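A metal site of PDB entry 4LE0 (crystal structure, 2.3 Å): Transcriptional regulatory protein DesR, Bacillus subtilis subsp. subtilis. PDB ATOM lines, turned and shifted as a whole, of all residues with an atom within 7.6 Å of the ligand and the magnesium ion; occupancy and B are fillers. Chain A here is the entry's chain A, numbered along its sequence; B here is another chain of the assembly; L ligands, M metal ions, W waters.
A beryllium atom (BE1) of the ligand is bound by the side-chain carboxylate (OD1) of Asp 58 (1.5 Å). A fluorine (F3) of the ligand sits at hydrogen-bond distance from the backbone NH (N) of Thr 85 (3.0 Å). F1 of the ligand is in hydrogen-bond range of N of Glu 60. The backbone NH of Ile 59 is in hydrogen-bond range of a fluorine (F1) of the ligand (3.0 Å). A fluorine (F3) of the ligand lies within hydrogen-bond range of the side-chain hydroxyl of Thr 85 (3.5 Å). The side-chain amino group (NZ) of Lys 106 lies within hydrogen-bond range of a fluorine (F3) of the ligand (2.7 Å). The side-chain hydroxyl of Thr 84 sits at hydrogen-bond distance from a fluorine (F1) of the ligand (2.6 Å).
N of Gln 14 of chain A lies within hydrogen-bond range of OE2 of Glu 12 (3.1 Å). The backbone carbonyl oxygen of Asp 58 sits close to the backbone NH of Gly 66 (3.5 Å). O of Phe 86 lies within hydrogen-bond range of OH of Tyr 103 (2.6 Å). The backbone NH of Asp 58 sits at hydrogen-bond distance from the backbone carbonyl oxygen of Ala 11 (2.9 Å). The backbone NH (N) of Thr 84 is in hydrogen-bond range of the backbone carbonyl oxygen (O) of Leu 104, 3.2 Å away. The backbone NH (N) of Phe 86 sits at hydrogen-bond distance from the side-chain hydroxyl (OG1) of Thr 84, 3.1 Å away. The backbone carbonyl oxygen (O) of Ile 59 is in hydrogen-bond range of the backbone NH (N) of Gly 66 (2.8 Å). The backbone NH (N) of Lys 106 sits at hydrogen-bond distance from the backbone carbonyl oxygen (O) of Thr 84 (2.8 Å).
CD2 of Phe 86 touches F1 of the ligand, 3.5 Å away. Hydrophobic or aromatic side chains within 4 Å of the ligand: Ile 59 and Phe 86. Within 4 Å of the ligand: Asp 58, Ile 59, Glu 60, Thr 84, Thr 85, Phe 86 and Lys 106.
Merely in contact with the magnesium ion: Glu 12. Four residues have an atom within 4 Å of the magnesium ion: Glu 12, Asp 13, Asp 58 and Glu 60. The nearest printed residue that does not touch the magnesium ion is Met 61 (4.3 Å).
The magnesium ion is bound by a fluorine (F2) of the ligand (2.0 Å), the side-chain carboxylate of Asp 58 (2.1 Å), the side-chain carboxylate of Asp 13 (2.1 Å), the backbone carbonyl oxygen of Glu 60 (2.1 Å), water W2 (2.1 Å) and water W1 (2.1 Å).
Water W1 bridges OE2 of Glu 12 (2.6 Å) and NZ of Lys 106 (3.0 Å). Water W3 lies within hydrogen-bond range of a fluorine (F3) of the ligand (3.0 Å) and the side-chain hydroxyl of Thr 85 (3.2 Å).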
ATOM      1  N   ALA A  11     -19.230   8.730 -17.329  1.00  0.00           N
ATOM      2  CA  ALA A  11     -19.646   7.824 -16.255  1.00  0.00           C
ATOM      3  C   ALA A  11     -21.053   7.330 -16.608  1.00  0.00           C
ATOM      4  O   ALA A  11     -21.988   8.129 -16.689  1.00  0.00           O
ATOM      5  CB  ALA A  11     -19.624   8.499 -14.897  1.00  0.00           C
ATOM      6  N   GLU A  12     -21.166   6.013 -16.881  1.00  0.00           N
ATOM      7  CA  GLU A  12     -22.405   5.360 -17.283  1.00  0.00           C
ATOM      8  C   GLU A  12     -22.276   3.887 -16.919  1.00  0.00           C
ATOM      9  O   GLU A  12     -21.322   3.244 -17.358  1.00  0.00           O
ATOM     10  CB  GLU A  12     -22.628   5.568 -18.809  1.00  0.00           C
ATOM     11  CG  GLU A  12     -23.732   4.734 -19.432  1.00  0.00           C
ATOM     12  CD  GLU A  12     -25.092   4.918 -18.806  1.00  0.00           C
ATOM     13  OE1 GLU A  12     -25.537   6.081 -18.697  1.00  0.00           O
ATOM     14  OE2 GLU A  12     -25.709   3.894 -18.419  1.00  0.00           O
ATOM     15  N   ASP A  13     -23.184   3.364 -16.071  1.00  0.00           N
ATOM     16  CA  ASP A  13     -23.115   1.973 -15.595  1.00  0.00           C
ATOM     17  C   ASP A  13     -23.435   0.920 -16.628  1.00  0.00           C
ATOM     18  O   ASP A  13     -22.897  -0.179 -16.539  1.00  0.00           O
ATOM     19  CB  ASP A  13     -23.901   1.765 -14.300  1.00  0.00           C
ATOM     20  CG  ASP A  13     -25.385   1.902 -14.426  1.00  0.00           C
ATOM     21  OD1 ASP A  13     -25.838   2.964 -14.879  1.00  0.00           O
ATOM     22  OD2 ASP A  13     -26.113   0.957 -14.024  1.00  0.00           O
ATOM     23  N   GLN A  14     -24.286   1.243 -17.614  1.00  0.00           N
ATOM     24  CA  GLN A  14     -24.648   0.296 -18.663  1.00  0.00           C
ATOM     25  C   GLN A  14     -23.554   0.361 -19.730  1.00  0.00           C
ATOM     26  O   GLN A  14     -23.475   1.343 -20.486  1.00  0.00           O
ATOM     27  CB  GLN A  14     -26.035   0.619 -19.245  1.00  0.00           C
ATOM     28  CG  GLN A  14     -27.137   0.676 -18.186  1.00  0.00           C
ATOM     29  CD  GLN A  14     -28.235  -0.330 -18.419  1.00  0.00           C
ATOM     30  OE1 GLN A  14     -29.364   0.034 -18.764  1.00  0.00           O
ATOM     31  NE2 GLN A  14     -27.999  -1.593 -18.134  1.00  0.00           N
ATOM     32  N   LEU A  17     -24.142   1.183 -23.496  1.00  0.00           N
ATOM     33  CA  LEU A  17     -24.415   2.611 -23.624  1.00  0.00           C
ATOM     34  C   LEU A  17     -23.150   3.436 -23.407  1.00  0.00           C
ATOM     35  O   LEU A  17     -22.929   4.401 -24.126  1.00  0.00           O
ATOM     36  CB  LEU A  17     -25.490   3.001 -22.589  1.00  0.00           C
ATOM     37  CG  LEU A  17     -26.916   2.405 -22.726  1.00  0.00           C
ATOM     38  CD1 LEU A  17     -26.990   0.926 -22.786  1.00  0.00           C
ATOM     39  CD2 LEU A  17     -27.811   2.873 -21.594  1.00  0.00           C
ATOM     40  N   THR A  38     -18.084   3.330 -14.763  1.00  0.00           N
ATOM     41  CA  THR A  38     -19.422   2.737 -14.591  1.00  0.00           C
ATOM     42  C   THR A  38     -20.059   3.063 -13.242  1.00  0.00           C
ATOM     43  O   THR A  38     -21.178   2.638 -12.989  1.00  0.00           O
ATOM     44  CB  THR A  38     -19.363   1.215 -14.827  1.00  0.00           C
ATOM     45  OG1 THR A  38     -18.364   0.674 -13.970  1.00  0.00           O
ATOM     46  CG2 THR A  38     -19.101   0.847 -16.298  1.00  0.00           C
ATOM     47  N   MET A  57     -22.133  12.583 -16.971  1.00  0.00           N
ATOM     48  CA  MET A  57     -22.536  11.883 -15.763  1.00  0.00           C
ATOM     49  C   MET A  57     -23.950  11.299 -15.764  1.00  0.00           C
ATOM     50  O   MET A  57     -24.957  12.024 -15.716  1.00  0.00           O
ATOM     51  CB  MET A  57     -22.367  12.833 -14.566  1.00  0.00           C
ATOM     52  CG  MET A  57     -22.436  12.174 -13.206  1.00  0.00           C
ATOM     53  SD  MET A  57     -20.862  11.497 -12.605  1.00  0.00           S
ATOM     54  CE  MET A  57     -20.014  13.028 -12.115  1.00  0.00           C
ATOM     55  N   ASP A  58     -24.020   9.995 -15.696  1.00  0.00           N
ATOM     56  CA  ASP A  58     -25.279   9.294 -15.524  1.00  0.00           C
ATOM     57  C   ASP A  58     -25.672   9.483 -14.040  1.00  0.00           C
ATOM     58  O   ASP A  58     -24.798   9.707 -13.208  1.00  0.00           O
ATOM     59  CB  ASP A  58     -25.072   7.804 -15.813  1.00  0.00           C
ATOM     60  CG  ASP A  58     -26.301   6.947 -15.654  1.00  0.00           C
ATOM     61  OD1 ASP A  58     -27.426   7.433 -15.979  1.00  0.00           O
ATOM     62  OD2 ASP A  58     -26.151   5.791 -15.256  1.00  0.00           O
ATOM     63  N   ILE A  59     -26.965   9.406 -13.703  1.00  0.00           N
ATOM     64  CA  ILE A  59     -27.354   9.540 -12.286  1.00  0.00           C
ATOM     65  C   ILE A  59     -27.293   8.173 -11.611  1.00  0.00           C
ATOM     66  O   ILE A  59     -26.445   7.929 -10.744  1.00  0.00           O
ATOM     67  CB  ILE A  59     -28.722  10.253 -12.051  1.00  0.00           C
ATOM     68  CG1 ILE A  59     -28.672  11.725 -12.492  1.00  0.00           C
ATOM     69  CG2 ILE A  59     -29.188  10.110 -10.546  1.00  0.00           C
ATOM     70  CD1 ILE A  59     -30.023  12.473 -12.536  1.00  0.00           C
ATOM     71  N   GLU A  60     -28.204   7.294 -11.989  1.00  0.00           N
ATOM     72  CA  GLU A  60     -28.333   6.006 -11.353  1.00  0.00           C
ATOM     73  C   GLU A  60     -27.276   5.025 -11.780  1.00  0.00           C
ATOM     74  O   GLU A  60     -27.263   4.542 -12.904  1.00  0.00           O
ATOM     75  CB  GLU A  60     -29.755   5.461 -11.481  1.00  0.00           C
ATOM     76  CG  GLU A  60     -30.768   6.348 -10.768  1.00  0.00           C
ATOM     77  CD  GLU A  60     -32.172   5.788 -10.654  1.00  0.00           C
ATOM     78  OE1 GLU A  60     -33.055   6.509 -10.137  1.00  0.00           O
ATOM     79  OE2 GLU A  60     -32.399   4.636 -11.107  1.00  0.00           O
ATOM     80  N   MET A  61     -26.315   4.819 -10.863  1.00  0.00           N
ATOM     81  CA  MET A  61     -25.176   3.915 -11.032  1.00  0.00           C
ATOM     82  C   MET A  61     -24.981   3.236  -9.688  1.00  0.00           C
ATOM     83  O   MET A  61     -25.363   3.832  -8.689  1.00  0.00           O
ATOM     84  CB  MET A  61     -23.901   4.694 -11.385  1.00  0.00           C
ATOM     85  CG  MET A  61     -24.041   5.560 -12.634  1.00  0.00           C
ATOM     86  SD  MET A  61     -22.459   6.177 -13.184  1.00  0.00           S
ATOM     87  CE  MET A  61     -22.311   7.627 -12.165  1.00  0.00           C
ATOM     88  N   PRO A  62     -24.409   2.013  -9.634  1.00  0.00           N
ATOM     89  CA  PRO A  62     -24.190   1.362  -8.322  1.00  0.00           C
ATOM     90  C   PRO A  62     -23.077   2.030  -7.507  1.00  0.00           C
ATOM     91  O   PRO A  62     -22.166   2.634  -8.073  1.00  0.00           O
ATOM     92  CB  PRO A  62     -23.844  -0.086  -8.682  1.00  0.00           C
ATOM     93  CG  PRO A  62     -24.085  -0.222 -10.167  1.00  0.00           C
ATOM     94  CD  PRO A  62     -23.934   1.147 -10.737  1.00  0.00           C
ATOM     95  N   THR A  65     -24.182   7.489  -6.761  1.00  0.00           N
ATOM     96  CA  THR A  65     -24.892   8.007  -7.939  1.00  0.00           C
ATOM     97  C   THR A  65     -24.103   9.161  -8.532  1.00  0.00           C
ATOM     98  O   THR A  65     -23.239   9.742  -7.849  1.00  0.00           O
ATOM     99  CB  THR A  65     -26.323   8.475  -7.589  1.00  0.00           C
ATOM    100  OG1 THR A  65     -26.261   9.731  -6.924  1.00  0.00           O
ATOM    101  CG2 THR A  65     -27.116   7.466  -6.778  1.00  0.00           C
ATOM    102  N   GLY A  66     -24.435   9.530  -9.762  1.00  0.00           N
ATOM    103  CA  GLY A  66     -23.832  10.668 -10.459  1.00  0.00           C
ATOM    104  C   GLY A  66     -24.098  11.995  -9.796  1.00  0.00           C
ATOM    105  O   GLY A  66     -23.321  12.930  -9.958  1.00  0.00           O
ATOM    106  N   ILE A  82     -24.992  16.270 -16.730  1.00  0.00           N
ATOM    107  CA  ILE A  82     -25.769  15.084 -16.359  1.00  0.00           C
ATOM    108  C   ILE A  82     -26.445  14.544 -17.645  1.00  0.00           C
ATOM    109  O   ILE A  82     -26.992  15.329 -18.436  1.00  0.00           O
ATOM    110  CB  ILE A  82     -26.787  15.394 -15.207  1.00  0.00           C
ATOM    111  CG1 ILE A  82     -26.102  15.684 -13.848  1.00  0.00           C
ATOM    112  CG2 ILE A  82     -27.843  14.294 -15.054  1.00  0.00           C
ATOM    113  CD1 ILE A  82     -25.437  14.477 -13.105  1.00  0.00           C
ATOM    114  N   LEU A  83     -26.375  13.227 -17.855  1.00  0.00           N
ATOM    115  CA  LEU A  83     -27.049  12.562 -18.967  1.00  0.00           C
ATOM    116  C   LEU A  83     -27.773  11.387 -18.337  1.00  0.00           C
ATOM    117  O   LEU A  83     -27.149  10.447 -17.861  1.00  0.00           O
ATOM    118  CB  LEU A  83     -26.085  12.138 -20.096  1.00  0.00           C
ATOM    119  CG  LEU A  83     -26.755  11.377 -21.275  1.00  0.00           C
ATOM    120  CD1 LEU A  83     -27.874  12.208 -21.952  1.00  0.00           C
ATOM    121  CD2 LEU A  83     -25.709  10.887 -22.276  1.00  0.00           C
ATOM    122  N   THR A  84     -29.112  11.466 -18.286  1.00  0.00           N
ATOM    123  CA  THR A  84     -29.950  10.488 -17.586  1.00  0.00           C
ATOM    124  C   THR A  84     -31.281  10.198 -18.276  1.00  0.00           C
ATOM    125  O   THR A  84     -31.747  10.988 -19.081  1.00  0.00           O
ATOM    126  CB  THR A  84     -30.171  11.019 -16.144  1.00  0.00           C
ATOM    127  OG1 THR A  84     -30.927  10.091 -15.360  1.00  0.00           O
ATOM    128  CG2 THR A  84     -30.839  12.412 -16.125  1.00  0.00           C
ATOM    129  N   THR A  85     -31.906   9.069 -17.885  1.00  0.00           N
ATOM    130  CA  THR A  85     -33.261   8.661 -18.303  1.00  0.00           C
ATOM    131  C   THR A  85     -34.281   9.542 -17.533  1.00  0.00           C
ATOM    132  O   THR A  85     -35.354   9.837 -18.043  1.00  0.00           O
ATOM    133  CB  THR A  85     -33.459   7.165 -17.908  1.00  0.00           C
ATOM    134  OG1 THR A  85     -32.606   6.356 -18.695  1.00  0.00           O
ATOM    135  CG2 THR A  85     -34.892   6.673 -18.087  1.00  0.00           C
ATOM    136  N   PHE A  86     -33.917   9.934 -16.298  1.00  0.00           N
ATOM    137  CA  PHE A  86     -34.778  10.626 -15.334  1.00  0.00           C
ATOM    138  C   PHE A  86     -34.959  12.127 -15.392  1.00  0.00           C
ATOM    139  O   PHE A  86     -34.062  12.905 -15.073  1.00  0.00           O
ATOM    140  CB  PHE A  86     -34.484  10.141 -13.891  1.00  0.00           C
ATOM    141  CG  PHE A  86     -34.281   8.644 -13.831  1.00  0.00           C
ATOM    142  CD1 PHE A  86     -35.371   7.779 -13.893  1.00  0.00           C
ATOM    143  CD2 PHE A  86     -33.004   8.108 -13.799  1.00  0.00           C
ATOM    144  CE1 PHE A  86     -35.178   6.388 -13.905  1.00  0.00           C
ATOM    145  CE2 PHE A  86     -32.812   6.728 -13.832  1.00  0.00           C
ATOM    146  CZ  PHE A  86     -33.899   5.881 -13.853  1.00  0.00           C
ATOM    147  N   TYR A  91     -34.025  15.569  -8.767  1.00  0.00           N
ATOM    148  CA  TYR A  91     -32.720  15.197  -9.336  1.00  0.00           C
ATOM    149  C   TYR A  91     -32.107  16.454  -9.973  1.00  0.00           C
ATOM    150  O   TYR A  91     -30.916  16.708  -9.810  1.00  0.00           O
ATOM    151  CB  TYR A  91     -32.903  14.102 -10.406  1.00  0.00           C
ATOM    152  CG  TYR A  91     -32.978  12.653  -9.934  1.00  0.00           C
ATOM    153  CD1 TYR A  91     -32.945  12.330  -8.576  1.00  0.00           C
ATOM    154  CD2 TYR A  91     -33.061  11.605 -10.851  1.00  0.00           C
ATOM    155  CE1 TYR A  91     -32.998  11.000  -8.145  1.00  0.00           C
ATOM    156  CE2 TYR A  91     -33.118  10.276 -10.430  1.00  0.00           C
ATOM    157  CZ  TYR A  91     -33.062   9.979  -9.082  1.00  0.00           C
ATOM    158  OH  TYR A  91     -33.080   8.649  -8.699  1.00  0.00           O
ATOM    159  N   TYR A 103     -27.782  19.367 -17.951  1.00  0.00           N
ATOM    160  CA  TYR A 103     -28.673  18.283 -17.587  1.00  0.00           C
ATOM    161  C   TYR A 103     -29.399  17.886 -18.863  1.00  0.00           C
ATOM    162  O   TYR A 103     -30.264  18.609 -19.365  1.00  0.00           O
ATOM    163  CB  TYR A 103     -29.630  18.688 -16.450  1.00  0.00           C
ATOM    164  CG  TYR A 103     -30.319  17.524 -15.759  1.00  0.00           C
ATOM    165  CD1 TYR A 103     -31.298  16.767 -16.413  1.00  0.00           C
ATOM    166  CD2 TYR A 103     -30.093  17.249 -14.418  1.00  0.00           C
ATOM    167  CE1 TYR A 103     -31.994  15.758 -15.763  1.00  0.00           C
ATOM    168  CE2 TYR A 103     -30.782  16.241 -13.749  1.00  0.00           C
ATOM    169  CZ  TYR A 103     -31.730  15.501 -14.428  1.00  0.00           C
ATOM    170  OH  TYR A 103     -32.432  14.522 -13.775  1.00  0.00           O
ATOM    171  N   LEU A 104     -28.983  16.754 -19.439  1.00  0.00           N
ATOM    172  CA  LEU A 104     -29.569  16.249 -20.676  1.00  0.00           C
ATOM    173  C   LEU A 104     -30.314  14.975 -20.407  1.00  0.00           C
ATOM    174  O   LEU A 104     -30.016  14.254 -19.465  1.00  0.00           O
ATOM    175  CB  LEU A 104     -28.486  15.994 -21.727  1.00  0.00           C
ATOM    176  CG  LEU A 104     -27.738  17.222 -22.324  1.00  0.00           C
ATOM    177  CD1 LEU A 104     -26.871  16.791 -23.477  1.00  0.00           C
ATOM    178  CD2 LEU A 104     -28.707  18.293 -22.838  1.00  0.00           C
ATOM    179  N   LYS A 106     -31.705  11.148 -21.852  1.00  0.00           N
ATOM    180  CA  LYS A 106     -31.338  10.097 -22.810  1.00  0.00           C
ATOM    181  C   LYS A 106     -32.375  10.062 -23.975  1.00  0.00           C
ATOM    182  O   LYS A 106     -32.210   9.342 -24.946  1.00  0.00           O
ATOM    183  CB  LYS A 106     -31.163   8.738 -22.096  1.00  0.00           C
ATOM    184  CG  LYS A 106     -29.811   8.645 -21.402  1.00  0.00           C
ATOM    185  CD  LYS A 106     -29.672   7.374 -20.597  1.00  0.00           C
ATOM    186  CE  LYS A 106     -28.390   7.370 -19.786  1.00  0.00           C
ATOM    187  NZ  LYS A 106     -28.293   6.158 -18.920  1.00  0.00           N
ATOM    188  N   GLN B  14     -35.097   5.686 -26.839  1.00  0.00           N
ATOM    189  CA  GLN B  14     -34.258   6.740 -26.278  1.00  0.00           C
ATOM    190  C   GLN B  14     -33.295   7.181 -27.378  1.00  0.00           C
ATOM    191  O   GLN B  14     -32.355   6.455 -27.712  1.00  0.00           O
ATOM    192  CB  GLN B  14     -33.531   6.250 -25.021  1.00  0.00           C
ATOM    193  CG  GLN B  14     -34.454   5.645 -23.938  1.00  0.00           C
ATOM    194  CD  GLN B  14     -35.352   6.636 -23.242  1.00  0.00           C
ATOM    195  OE1 GLN B  14     -36.580   6.611 -23.423  1.00  0.00           O
ATOM    196  NE2 GLN B  14     -34.759   7.548 -22.499  1.00  0.00           N
ATOM    197  N   LEU B  17     -29.402   7.170 -27.087  1.00  0.00           N
ATOM    198  CA  LEU B  17     -28.949   5.784 -27.188  1.00  0.00           C
ATOM    199  C   LEU B  17     -29.074   5.247 -28.612  1.00  0.00           C
ATOM    200  O   LEU B  17     -28.180   4.543 -29.068  1.00  0.00           O
ATOM    201  CB  LEU B  17     -29.752   4.912 -26.199  1.00  0.00           C
ATOM    202  CG  LEU B  17     -29.726   5.311 -24.689  1.00  0.00           C
ATOM    203  CD1 LEU B  17     -30.546   4.420 -23.877  1.00  0.00           C
ATOM    204  CD2 LEU B  17     -28.290   5.653 -24.141  1.00  0.00           C
ATOM    205  N   ASP B 107     -26.200  -4.020 -20.505  1.00  0.00           N
ATOM    206  CA  ASP B 107     -25.058  -4.107 -19.623  1.00  0.00           C
ATOM    207  C   ASP B 107     -23.978  -5.043 -20.180  1.00  0.00           C
ATOM    208  O   ASP B 107     -22.986  -5.306 -19.505  1.00  0.00           O
ATOM    209  CB  ASP B 107     -25.469  -4.428 -18.184  1.00  0.00           C
ATOM    210  CG  ASP B 107     -24.796  -3.489 -17.192  1.00  0.00           C
ATOM    211  OD1 ASP B 107     -23.534  -3.304 -17.287  1.00  0.00           O
ATOM    212  OD2 ASP B 107     -25.517  -2.905 -16.342  1.00  0.00           O
HETATM  213 BE1  LIG L   1     -28.793   7.119 -15.522  1.00  0.00          BE
HETATM  214  F1  LIG L   1     -29.537   8.105 -14.392  1.00  0.00           F
HETATM  215  F2  LIG L   1     -28.959   5.544 -14.966  1.00  0.00           F
HETATM  216  F3  LIG L   1     -29.763   7.194 -16.891  1.00  0.00           F
HETATM  217 MG    MG M   1     -27.487   4.230 -14.961  1.00  0.00          MG
HETATM  218  O   HOH W   1     -27.860   3.840 -17.040  1.00  0.00           O
HETATM  219  O   HOH W   2     -29.122   2.959 -14.408  1.00  0.00           O
HETATM  220  O   HOH W   3     -31.281   4.733 -16.242  1.00  0.00           O
